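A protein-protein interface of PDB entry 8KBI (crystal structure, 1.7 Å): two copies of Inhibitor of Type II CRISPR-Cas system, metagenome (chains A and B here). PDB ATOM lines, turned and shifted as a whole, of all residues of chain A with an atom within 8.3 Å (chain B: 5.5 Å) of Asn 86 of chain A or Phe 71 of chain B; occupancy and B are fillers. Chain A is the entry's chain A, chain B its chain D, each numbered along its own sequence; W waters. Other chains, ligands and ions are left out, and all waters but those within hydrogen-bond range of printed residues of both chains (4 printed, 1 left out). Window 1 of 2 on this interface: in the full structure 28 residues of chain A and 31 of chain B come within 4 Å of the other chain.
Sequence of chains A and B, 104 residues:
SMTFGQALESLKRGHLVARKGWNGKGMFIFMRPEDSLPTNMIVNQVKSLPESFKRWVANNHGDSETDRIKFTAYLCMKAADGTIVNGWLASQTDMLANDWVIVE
The backbone NH (N) of Ile 84 of chain A is in hydrogen-bond range of the backbone carbonyl oxygen (O) of Lys 70 of chain B.
OG of Ser 48 of chain A sits at hydrogen-bond distance from O of Pro 33 of chain B (3.1 Å).
The backbone carbonyl oxygen (O) of Ile 84 of chain A lies within hydrogen-bond range of the backbone NH (N) of Thr 72 of chain B (3.0 Å).
The backbone carbonyl oxygen (O) of Phe 30 of chain A sits at hydrogen-bond distance from the backbone NH (N) of Cys 76 of chain A (2.9 Å).
The side-chain hydroxyl of Tyr 74 of chain B lies close to the side-chain amide oxygen of Asn 86 of chain B, at 3.3 Å.
OE2 of Glu 34 of chain B is in salt-bridge range of NZ of Lys 70 of chain B, at 3.9 Å.
N of Phe 71 of chain B lies within hydrogen-bond range of O of Asp 35 of chain B (2.7 Å).
OD1 of Asn 86 of chain A sits at hydrogen-bond distance from NH1 of Arg 32 of chain A.
The backbone carbonyl oxygen (O) of Leu 75 of chain A lies within hydrogen-bond range of the backbone NH (N) of Gly 87 of chain A (2.9 Å).
Among the printed residues, merely in contact across the chains: Phe 30 of chain A with Phe 53 of chain B (3.8 Å), Arg 32 of chain A with Leu 49 of chain B (3.4 Å), Ser 48 of chain A with Asp 35 of chain B (3.6 Å), Tyr 74 of chain A with Asn 86 of chain B (3.4 Å), Thr 83 of chain A with Lys 70 of chain B (3.4 Å), Thr 83 of chain A with Thr 72 of chain B (3.7 Å), Ile 84 of chain A with Phe 53 of chain B (3.8 Å), Ile 84 of chain A with Ile 69 of chain B (3.5 Å), Ile 84 of chain A with Phe 71 of chain B (3.3 Å), Val 85 of chain A with Thr 72 of chain B (3.8 Å), Asn 86 of chain A with Phe 71 of chain B (3.6 Å), Asn 86 of chain A with Tyr 74 of chain B (3.4 Å) and Gly 87 of chain A with Gly 87 of chain B (3.4 Å).
Printed residues of chain B within 4 Å of Ile 84 of chain A: Phe 53 (3.8 Å), Ile 69 (3.5 Å), Lys 70 (2.9 Å), Phe 71 (3.3 Å) and Thr 72 (3.0 Å).
Asn 86 of chain A touches just these residues of chain B: Phe 71 (3.6 Å) and Tyr 74 (3.4 Å).
Printed residues of chain A within 4 Å of Phe 53 of chain B: Phe 30 (3.8 Å) and Ile 84 (3.8 Å).
Phe 71 of chain B touches two residues of chain A.
Of the printed residues of chain A, Asn 86 of chain B touches Tyr 74 (3.4 Å).
The nearest residue of chain B that does not touch Asn 86 of chain A is Gly 87 of chain B (4.3 Å).
The nearest residue of chain A that does not touch Phe 71 of chain B is Arg 32 of chain A (4.3 Å).
Hydrophobic or aromatic side chains of chain B within 4 Å of the printed part of chain A: Pro 33, Leu 49, Phe 53, Ile 69, Phe 71 and Tyr 74.
Of the 16 printed residues of chain A, 9 touch a printed residue of chain B.
Tyr 74 of chain A touches Asn 86 of chain B, and with the chains exchanged Asn 86 of chain A touches Tyr 74 of chain B.
Gly 87 of chain A touches its own counterpart, Gly 87 of chain B.
Positions printed for both chains: 74, 86 and 87.
Of the 16 pairs that touch across the chains among the printed residues, 3 have their exchanged pair printed and touching as well.
Water W3 bridges OG of Ser 48 of chain A and O of Glu 34 of chain B.
Water W2 bridges the side-chain hydroxyl (OH) of Tyr 74 of chain B and the side-chain hydroxyl (OH) of Tyr 74 of chain A.
Water W4 lies within hydrogen-bond range of O of Thr 72 of chain B (2.7 Å), O of Ile 84 of chain A (2.8 Å) and N of Asn 86 of chain A (2.9 Å).
Water W1 bridges O of Gly 82 of chain A (2.9 Å) and N of Lys 70 of chain B (3.0 Å).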
ATOM      1  N   PHE A  30      13.556 -19.084 -22.282  1.00  0.00           N
ATOM      2  CA  PHE A  30      12.294 -19.781 -22.491  1.00  0.00           C
ATOM      3  C   PHE A  30      11.789 -20.313 -21.160  1.00  0.00           C
ATOM      4  O   PHE A  30      12.550 -20.459 -20.205  1.00  0.00           O
ATOM      5  CB  PHE A  30      12.434 -20.919 -23.518  1.00  0.00           C
ATOM      6  CG  PHE A  30      13.449 -21.960 -23.160  1.00  0.00           C
ATOM      7  CD1 PHE A  30      14.804 -21.760 -23.408  1.00  0.00           C
ATOM      8  CD2 PHE A  30      13.047 -23.165 -22.592  1.00  0.00           C
ATOM      9  CE1 PHE A  30      15.750 -22.761 -23.062  1.00  0.00           C
ATOM     10  CE2 PHE A  30      13.972 -24.139 -22.276  1.00  0.00           C
ATOM     11  CZ  PHE A  30      15.310 -23.935 -22.497  1.00  0.00           C
ATOM     12  N   ARG A  32      10.116 -23.389 -18.874  1.00  0.00           N
ATOM     13  CA  ARG A  32       9.778 -24.788 -18.689  1.00  0.00           C
ATOM     14  C   ARG A  32       8.616 -24.886 -17.709  1.00  0.00           C
ATOM     15  O   ARG A  32       8.633 -24.244 -16.633  1.00  0.00           O
ATOM     16  CB  ARG A  32      10.985 -25.603 -18.188  1.00  0.00           C
ATOM     17  CG  ARG A  32      12.143 -25.598 -19.203  1.00  0.00           C
ATOM     18  CD  ARG A  32      13.281 -26.495 -18.721  1.00  0.00           C
ATOM     19  NE  ARG A  32      12.976 -27.910 -18.870  1.00  0.00           N
ATOM     20  CZ  ARG A  32      13.885 -28.852 -18.685  1.00  0.00           C
ATOM     21  NH1 ARG A  32      15.106 -28.499 -18.337  1.00  0.00           N
ATOM     22  NH2 ARG A  32      13.578 -30.124 -18.846  1.00  0.00           N
ATOM     23  N   SER A  48      20.817 -36.188 -12.269  1.00  0.00           N
ATOM     24  CA  SER A  48      21.063 -34.790 -12.154  1.00  0.00           C
ATOM     25  C   SER A  48      20.427 -34.447 -10.817  1.00  0.00           C
ATOM     26  O   SER A  48      19.962 -33.380 -10.637  1.00  0.00           O
ATOM     27  CB  SER A  48      20.708 -33.881 -13.328  1.00  0.00           C
ATOM     28  OG  SER A  48      21.797 -33.663 -14.184  1.00  0.00           O
ATOM     29  N   TYR A  74       9.722 -22.509 -14.406  1.00  0.00           N
ATOM     30  CA  TYR A  74      10.936 -21.716 -14.209  1.00  0.00           C
ATOM     31  C   TYR A  74      11.493 -21.332 -15.579  1.00  0.00           C
ATOM     32  O   TYR A  74      11.080 -21.882 -16.606  1.00  0.00           O
ATOM     33  CB  TYR A  74      11.990 -22.466 -13.368  1.00  0.00           C
ATOM     34  CG  TYR A  74      12.461 -23.791 -13.987  1.00  0.00           C
ATOM     35  CD1 TYR A  74      11.684 -24.938 -13.885  1.00  0.00           C
ATOM     36  CD2 TYR A  74      13.681 -23.888 -14.642  1.00  0.00           C
ATOM     37  CE1 TYR A  74      12.082 -26.148 -14.445  1.00  0.00           C
ATOM     38  CE2 TYR A  74      14.110 -25.124 -15.184  1.00  0.00           C
ATOM     39  CZ  TYR A  74      13.297 -26.235 -15.083  1.00  0.00           C
ATOM     40  OH  TYR A  74      13.707 -27.449 -15.624  1.00  0.00           O
ATOM     41  N   LEU A  75      12.392 -20.341 -15.581  1.00  0.00           N
ATOM     42  CA  LEU A  75      12.966 -19.801 -16.817  1.00  0.00           C
ATOM     43  C   LEU A  75      14.369 -20.372 -17.045  1.00  0.00           C
ATOM     44  O   LEU A  75      15.109 -20.643 -16.101  1.00  0.00           O
ATOM     45  CB  LEU A  75      13.020 -18.257 -16.761  1.00  0.00           C
ATOM     46  CG  LEU A  75      11.635 -17.619 -16.582  1.00  0.00           C
ATOM     47  CD1 LEU A  75      11.725 -16.100 -16.687  1.00  0.00           C
ATOM     48  CD2 LEU A  75      10.684 -18.155 -17.655  1.00  0.00           C
ATOM     49  N   CYS A  76      14.717 -20.522 -18.326  1.00  0.00           N
ATOM     50  CA  CYS A  76      15.999 -21.037 -18.728  1.00  0.00           C
ATOM     51  C   CYS A  76      16.595 -20.224 -19.848  1.00  0.00           C
ATOM     52  O   CYS A  76      15.888 -19.561 -20.524  1.00  0.00           O
ATOM     53  CB  CYS A  76      15.851 -22.454 -19.240  1.00  0.00           C
ATOM     54  SG  CYS A  76      15.000 -23.562 -18.140  1.00  0.00           S
ATOM     55  N   MET A  77      17.901 -20.328 -20.026  1.00  0.00           N
ATOM     56  CA  MET A  77      18.578 -19.623 -21.085  1.00  0.00           C
ATOM     57  C   MET A  77      19.400 -20.461 -22.012  1.00  0.00           C
ATOM     58  O   MET A  77      20.104 -21.331 -21.527  1.00  0.00           O
ATOM     59  CB  MET A  77      19.583 -18.629 -20.499  1.00  0.00           C
ATOM     60  CG  MET A  77      20.284 -17.815 -21.569  1.00  0.00           C
ATOM     61  SD  MET A  77      21.530 -16.490 -20.874  1.00  0.00           S
ATOM     62  CE  MET A  77      20.450 -15.020 -21.576  1.00  0.00           C
ATOM     63  N   LYS A  78      19.300 -20.245 -23.313  1.00  0.00           N
ATOM     64  CA  LYS A  78      20.202 -20.882 -24.248  1.00  0.00           C
ATOM     65  C   LYS A  78      21.288 -19.849 -24.341  1.00  0.00           C
ATOM     66  O   LYS A  78      21.094 -18.801 -24.894  1.00  0.00           O
ATOM     67  CB  LYS A  78      19.574 -21.141 -25.597  1.00  0.00           C
ATOM     68  CG  LYS A  78      20.514 -21.779 -26.605  1.00  0.00           C
ATOM     69  CD  LYS A  78      20.910 -20.749 -27.637  1.00  0.00           C
ATOM     70  CE  LYS A  78      22.265 -21.029 -28.204  1.00  0.00           C
ATOM     71  NZ  LYS A  78      22.926 -19.738 -28.453  1.00  0.00           N
ATOM     72  N   GLY A  82      26.077 -21.897 -26.422  1.00  0.00           N
ATOM     73  CA  GLY A  82      25.250 -23.012 -26.810  1.00  0.00           C
ATOM     74  C   GLY A  82      24.767 -23.898 -25.683  1.00  0.00           C
ATOM     75  O   GLY A  82      23.962 -24.793 -25.938  1.00  0.00           O
ATOM     76  N   THR A  83      25.200 -23.671 -24.450  1.00  0.00           N
ATOM     77  CA  THR A  83      24.722 -24.478 -23.340  1.00  0.00           C
ATOM     78  C   THR A  83      23.364 -23.966 -22.863  1.00  0.00           C
ATOM     79  O   THR A  83      22.935 -22.855 -23.191  1.00  0.00           O
ATOM     80  CB  THR A  83      25.721 -24.452 -22.185  1.00  0.00           C
ATOM     81  OG1 THR A  83      25.903 -23.086 -21.796  1.00  0.00           O
ATOM     82  CG2 THR A  83      27.061 -25.034 -22.587  1.00  0.00           C
ATOM     83  N   ILE A  84      22.693 -24.784 -22.064  1.00  0.00           N
ATOM     84  CA  ILE A  84      21.398 -24.437 -21.468  1.00  0.00           C
ATOM     85  C   ILE A  84      21.600 -24.230 -19.980  1.00  0.00           C
ATOM     86  O   ILE A  84      22.109 -25.120 -19.279  1.00  0.00           O
ATOM     87  CB  ILE A  84      20.338 -25.526 -21.714  1.00  0.00           C
ATOM     88  CG1 ILE A  84      20.226 -25.870 -23.209  1.00  0.00           C
ATOM     89  CG2 ILE A  84      18.962 -25.066 -21.198  1.00  0.00           C
ATOM     90  CD1 ILE A  84      19.862 -24.678 -24.104  1.00  0.00           C
ATOM     91  N   VAL A  85      21.182 -23.073 -19.501  1.00  0.00           N
ATOM     92  CA  VAL A  85      21.179 -22.742 -18.078  1.00  0.00           C
ATOM     93  C   VAL A  85      19.754 -22.848 -17.572  1.00  0.00           C
ATOM     94  O   VAL A  85      18.920 -22.009 -17.897  1.00  0.00           O
ATOM     95  CB  VAL A  85      21.711 -21.336 -17.805  1.00  0.00           C
ATOM     96  CG1 VAL A  85      21.636 -21.111 -16.300  1.00  0.00           C
ATOM     97  CG2 VAL A  85      23.125 -21.157 -18.317  1.00  0.00           C
ATOM     98  N   ASN A  86      19.469 -23.887 -16.786  1.00  0.00           N
ATOM     99  CA  ASN A  86      18.214 -23.988 -16.051  1.00  0.00           C
ATOM    100  C   ASN A  86      18.258 -22.963 -14.925  1.00  0.00           C
ATOM    101  O   ASN A  86      19.213 -22.942 -14.140  1.00  0.00           O
ATOM    102  CB  ASN A  86      18.047 -25.391 -15.459  1.00  0.00           C
ATOM    103  CG  ASN A  86      17.674 -26.445 -16.494  1.00  0.00           C
ATOM    104  OD1 ASN A  86      16.573 -26.442 -17.061  1.00  0.00           O
ATOM    105  ND2 ASN A  86      18.608 -27.359 -16.751  1.00  0.00           N
ATOM    106  N   GLY A  87      17.288 -22.053 -14.900  1.00  0.00           N
ATOM    107  CA  GLY A  87      17.227 -21.106 -13.812  1.00  0.00           C
ATOM    108  C   GLY A  87      17.769 -19.744 -14.158  1.00  0.00           C
ATOM    109  O   GLY A  87      18.539 -19.163 -13.384  1.00  0.00           O
ATOM    110  N   TRP A  88      17.419 -19.253 -15.359  1.00  0.00           N
ATOM    111  CA  TRP A  88      17.821 -17.912 -15.753  1.00  0.00           C
ATOM    112  C   TRP A  88      17.260 -16.901 -14.772  1.00  0.00           C
ATOM    113  O   TRP A  88      16.149 -17.044 -14.272  1.00  0.00           O
ATOM    114  CB  TRP A  88      17.304 -17.590 -17.165  1.00  0.00           C
ATOM    115  CG  TRP A  88      17.565 -16.172 -17.599  1.00  0.00           C
ATOM    116  CD1 TRP A  88      18.715 -15.698 -18.119  1.00  0.00           C
ATOM    117  CD2 TRP A  88      16.647 -15.073 -17.583  1.00  0.00           C
ATOM    118  NE1 TRP A  88      18.605 -14.367 -18.409  1.00  0.00           N
ATOM    119  CE2 TRP A  88      17.341 -13.946 -18.081  1.00  0.00           C
ATOM    120  CE3 TRP A  88      15.306 -14.917 -17.166  1.00  0.00           C
ATOM    121  CZ2 TRP A  88      16.740 -12.680 -18.203  1.00  0.00           C
ATOM    122  CZ3 TRP A  88      14.713 -13.664 -17.269  1.00  0.00           C
ATOM    123  CH2 TRP A  88      15.426 -12.553 -17.786  1.00  0.00           C
ATOM    124  N   LEU A  89      18.046 -15.919 -14.456  1.00  0.00           N
ATOM    125  CA  LEU A  89      17.587 -14.872 -13.553  1.00  0.00           C
ATOM    126  C   LEU A  89      17.795 -13.522 -14.246  1.00  0.00           C
ATOM    127  O   LEU A  89      18.665 -13.359 -15.121  1.00  0.00           O
ATOM    128  CB  LEU A  89      18.306 -15.078 -12.175  1.00  0.00           C
ATOM    129  CG  LEU A  89      17.933 -16.348 -11.334  1.00  0.00           C
ATOM    130  CD1 LEU A  89      18.830 -16.711 -10.109  1.00  0.00           C
ATOM    131  CD2 LEU A  89      16.559 -16.191 -10.711  1.00  0.00           C
ATOM    132  N   PRO B  33      23.969 -31.291 -10.976  1.00  0.00           N
ATOM    133  CA  PRO B  33      25.204 -31.218 -11.759  1.00  0.00           C
ATOM    134  C   PRO B  33      24.909 -31.094 -13.247  1.00  0.00           C
ATOM    135  O   PRO B  33      23.795 -31.309 -13.704  1.00  0.00           O
ATOM    136  CB  PRO B  33      25.877 -32.560 -11.461  1.00  0.00           C
ATOM    137  CG  PRO B  33      24.701 -33.486 -11.250  1.00  0.00           C
ATOM    138  CD  PRO B  33      23.629 -32.667 -10.562  1.00  0.00           C
ATOM    139  N   GLU B  34      25.971 -30.799 -13.989  1.00  0.00           N
ATOM    140  CA  GLU B  34      25.934 -30.705 -15.446  1.00  0.00           C
ATOM    141  C   GLU B  34      25.495 -32.031 -16.064  1.00  0.00           C
ATOM    142  O   GLU B  34      25.761 -33.111 -15.526  1.00  0.00           O
ATOM    143  CB  GLU B  34      27.325 -30.325 -15.923  1.00  0.00           C
ATOM    144  CG  GLU B  34      27.588 -30.241 -17.371  1.00  0.00           C
ATOM    145  CD  GLU B  34      29.075 -30.120 -17.657  1.00  0.00           C
ATOM    146  OE1 GLU B  34      29.675 -29.107 -17.236  1.00  0.00           O
ATOM    147  OE2 GLU B  34      29.631 -31.022 -18.325  1.00  0.00           O
ATOM    148  N   ASP B  35      24.803 -31.950 -17.203  1.00  0.00           N
ATOM    149  CA  ASP B  35      24.457 -33.168 -17.933  1.00  0.00           C
ATOM    150  C   ASP B  35      24.451 -32.836 -19.411  1.00  0.00           C
ATOM    151  O   ASP B  35      24.109 -31.728 -19.786  1.00  0.00           O
ATOM    152  CB  ASP B  35      23.102 -33.699 -17.512  1.00  0.00           C
ATOM    153  CG  ASP B  35      22.891 -35.145 -17.916  1.00  0.00           C
ATOM    154  OD1 ASP B  35      23.827 -35.774 -18.462  1.00  0.00           O
ATOM    155  OD2 ASP B  35      21.774 -35.639 -17.693  1.00  0.00           O
ATOM    156  N   SER B  36      24.813 -33.800 -20.257  1.00  0.00           N
ATOM    157  CA  SER B  36      24.921 -33.572 -21.697  1.00  0.00           C
ATOM    158  C   SER B  36      24.063 -34.629 -22.374  1.00  0.00           C
ATOM    159  O   SER B  36      24.308 -35.816 -22.173  1.00  0.00           O
ATOM    160  CB  SER B  36      26.393 -33.658 -22.146  1.00  0.00           C
ATOM    161  OG  SER B  36      26.576 -33.866 -23.558  1.00  0.00           O
ATOM    162  N   LEU B  37      23.031 -34.204 -23.139  1.00  0.00           N
ATOM    163  CA  LEU B  37      22.024 -35.140 -23.651  1.00  0.00           C
ATOM    164  C   LEU B  37      21.919 -35.076 -25.168  1.00  0.00           C
ATOM    165  O   LEU B  37      22.053 -33.996 -25.737  1.00  0.00           O
ATOM    166  CB  LEU B  37      20.646 -34.834 -23.074  1.00  0.00           C
ATOM    167  CG  LEU B  37      20.470 -34.838 -21.559  1.00  0.00           C
ATOM    168  CD1 LEU B  37      19.074 -34.293 -21.250  1.00  0.00           C
ATOM    169  CD2 LEU B  37      20.638 -36.248 -21.062  1.00  0.00           C
ATOM    170  N   ILE B  42      16.099 -34.796 -26.583  1.00  0.00           N
ATOM    171  CA  ILE B  42      15.548 -33.485 -26.249  1.00  0.00           C
ATOM    172  C   ILE B  42      14.286 -33.230 -27.051  1.00  0.00           C
ATOM    173  O   ILE B  42      13.257 -32.790 -26.525  1.00  0.00           O
ATOM    174  CB  ILE B  42      16.584 -32.382 -26.518  1.00  0.00           C
ATOM    175  CG1 ILE B  42      17.778 -32.541 -25.576  1.00  0.00           C
ATOM    176  CG2 ILE B  42      15.931 -31.021 -26.425  1.00  0.00           C
ATOM    177  CD1 ILE B  42      17.460 -32.164 -24.153  1.00  0.00           C
ATOM    178  N   LEU B  49       9.603 -29.231 -21.924  1.00  0.00           N
ATOM    179  CA  LEU B  49      10.235 -28.258 -22.790  1.00  0.00           C
ATOM    180  C   LEU B  49       9.173 -27.683 -23.713  1.00  0.00           C
ATOM    181  O   LEU B  49       8.287 -28.428 -24.144  1.00  0.00           O
ATOM    182  CB  LEU B  49      11.356 -28.896 -23.633  1.00  0.00           C
ATOM    183  CG  LEU B  49      12.618 -29.320 -22.876  1.00  0.00           C
ATOM    184  CD1 LEU B  49      13.604 -30.032 -23.837  1.00  0.00           C
ATOM    185  CD2 LEU B  49      13.274 -28.105 -22.212  1.00  0.00           C
ATOM    186  N   PHE B  53      11.190 -24.491 -28.311  1.00  0.00           N
ATOM    187  CA  PHE B  53      12.583 -24.863 -28.064  1.00  0.00           C
ATOM    188  C   PHE B  53      12.928 -26.194 -28.722  1.00  0.00           C
ATOM    189  O   PHE B  53      14.027 -26.362 -29.269  1.00  0.00           O
ATOM    190  CB  PHE B  53      12.844 -24.937 -26.556  1.00  0.00           C
ATOM    191  CG  PHE B  53      14.235 -25.380 -26.218  1.00  0.00           C
ATOM    192  CD1 PHE B  53      15.307 -24.543 -26.387  1.00  0.00           C
ATOM    193  CD2 PHE B  53      14.461 -26.685 -25.812  1.00  0.00           C
ATOM    194  CE1 PHE B  53      16.590 -24.973 -26.077  1.00  0.00           C
ATOM    195  CE2 PHE B  53      15.730 -27.122 -25.509  1.00  0.00           C
ATOM    196  CZ  PHE B  53      16.804 -26.272 -25.649  1.00  0.00           C
ATOM    197  N   ILE B  69      23.479 -31.561 -26.356  1.00  0.00           N
ATOM    198  CA  ILE B  69      23.326 -30.259 -25.754  1.00  0.00           C
ATOM    199  C   ILE B  69      23.650 -30.373 -24.296  1.00  0.00           C
ATOM    200  O   ILE B  69      23.152 -31.242 -23.629  1.00  0.00           O
ATOM    201  CB  ILE B  69      21.918 -29.708 -25.916  1.00  0.00           C
ATOM    202  CG1 ILE B  69      21.637 -29.457 -27.391  1.00  0.00           C
ATOM    203  CG2 ILE B  69      21.727 -28.417 -25.155  1.00  0.00           C
ATOM    204  CD1 ILE B  69      20.341 -28.743 -27.653  1.00  0.00           C
ATOM    205  N   LYS B  70      24.496 -29.487 -23.826  1.00  0.00           N
ATOM    206  CA  LYS B  70      24.882 -29.472 -22.454  1.00  0.00           C
ATOM    207  C   LYS B  70      24.068 -28.582 -21.559  1.00  0.00           C
ATOM    208  O   LYS B  70      23.848 -27.445 -21.890  1.00  0.00           O
ATOM    209  CB  LYS B  70      26.328 -29.046 -22.360  1.00  0.00           C
ATOM    210  CG  LYS B  70      26.899 -29.070 -20.954  1.00  0.00           C
ATOM    211  CD  LYS B  70      28.344 -28.619 -20.931  1.00  0.00           C
ATOM    212  CE  LYS B  70      29.221 -29.580 -21.712  1.00  0.00           C
ATOM    213  NZ  LYS B  70      30.658 -29.237 -21.591  1.00  0.00           N
ATOM    214  N   PHE B  71      23.613 -29.129 -20.442  1.00  0.00           N
ATOM    215  CA  PHE B  71      22.898 -28.369 -19.457  1.00  0.00           C
ATOM    216  C   PHE B  71      23.861 -28.104 -18.303  1.00  0.00           C
ATOM    217  O   PHE B  71      24.309 -29.030 -17.690  1.00  0.00           O
ATOM    218  CB  PHE B  71      21.693 -29.132 -18.978  1.00  0.00           C
ATOM    219  CG  PHE B  71      20.641 -29.323 -20.028  1.00  0.00           C
ATOM    220  CD1 PHE B  71      20.782 -30.276 -21.012  1.00  0.00           C
ATOM    221  CD2 PHE B  71      19.510 -28.556 -20.018  1.00  0.00           C
ATOM    222  CE1 PHE B  71      19.827 -30.439 -21.979  1.00  0.00           C
ATOM    223  CE2 PHE B  71      18.540 -28.723 -20.976  1.00  0.00           C
ATOM    224  CZ  PHE B  71      18.703 -29.657 -21.961  1.00  0.00           C
ATOM    225  N   THR B  72      24.175 -26.843 -18.033  1.00  0.00           N
ATOM    226  CA  THR B  72      25.124 -26.463 -16.986  1.00  0.00           C
ATOM    227  C   THR B  72      24.604 -26.884 -15.605  1.00  0.00           C
ATOM    228  O   THR B  72      23.412 -27.090 -15.408  1.00  0.00           O
ATOM    229  CB  THR B  72      25.302 -24.937 -16.972  1.00  0.00           C
ATOM    230  OG1 THR B  72      24.130 -24.352 -16.390  1.00  0.00           O
ATOM    231  CG2 THR B  72      25.439 -24.356 -18.335  1.00  0.00           C
ATOM    232  N   ALA B  73      25.509 -26.984 -14.631  1.00  0.00           N
ATOM    233  CA  ALA B  73      25.048 -27.179 -13.262  1.00  0.00           C
ATOM    234  C   ALA B  73      24.253 -25.978 -12.798  1.00  0.00           C
ATOM    235  O   ALA B  73      24.446 -24.872 -13.290  1.00  0.00           O
ATOM    236  CB  ALA B  73      26.231 -27.360 -12.296  1.00  0.00           C
ATOM    237  N   TYR B  74      23.369 -26.194 -11.829  1.00  0.00           N
ATOM    238  CA  TYR B  74      22.577 -25.072 -11.316  1.00  0.00           C
ATOM    239  C   TYR B  74      22.055 -25.388  -9.929  1.00  0.00           C
ATOM    240  O   TYR B  74      22.142 -26.516  -9.458  1.00  0.00           O
ATOM    241  CB  TYR B  74      21.415 -24.734 -12.255  1.00  0.00           C
ATOM    242  CG  TYR B  74      20.455 -25.872 -12.500  1.00  0.00           C
ATOM    243  CD1 TYR B  74      20.792 -26.924 -13.363  1.00  0.00           C
ATOM    244  CD2 TYR B  74      19.180 -25.877 -11.933  1.00  0.00           C
ATOM    245  CE1 TYR B  74      19.925 -27.959 -13.593  1.00  0.00           C
ATOM    246  CE2 TYR B  74      18.309 -26.930 -12.160  1.00  0.00           C
ATOM    247  CZ  TYR B  74      18.680 -27.951 -13.008  1.00  0.00           C
ATOM    248  OH  TYR B  74      17.810 -28.995 -13.261  1.00  0.00           O
ATOM    249  N   ASN B  86      13.552 -25.256  -9.558  1.00  0.00           N
ATOM    250  CA  ASN B  86      14.794 -25.244 -10.333  1.00  0.00           C
ATOM    251  C   ASN B  86      15.220 -23.802 -10.581  1.00  0.00           C
ATOM    252  O   ASN B  86      14.420 -23.009 -11.088  1.00  0.00           O
ATOM    253  CB  ASN B  86      14.606 -25.945 -11.673  1.00  0.00           C
ATOM    254  CG  ASN B  86      14.455 -27.433 -11.531  1.00  0.00           C
ATOM    255  OD1 ASN B  86      15.393 -28.122 -11.152  1.00  0.00           O
ATOM    256  ND2 ASN B  86      13.274 -27.936 -11.830  1.00  0.00           N
ATOM    257  N   GLY B  87      16.477 -23.472 -10.265  1.00  0.00           N
ATOM    258  CA  GLY B  87      17.013 -22.159 -10.564  1.00  0.00           C
ATOM    259  C   GLY B  87      16.849 -21.224  -9.380  1.00  0.00           C
ATOM    260  O   GLY B  87      16.344 -20.113  -9.517  1.00  0.00           O
HETATM  261  O   HOH W   1      25.085 -27.419 -25.862  1.00  0.00           O
HETATM  262  O   HOH W   2      15.606 -29.309 -14.811  1.00  0.00           O
HETATM  263  O   HOH W   3      23.900 -35.205 -14.313  1.00  0.00           O
HETATM  264  O   HOH W   4      21.281 -26.094 -16.790  1.00  0.00           O
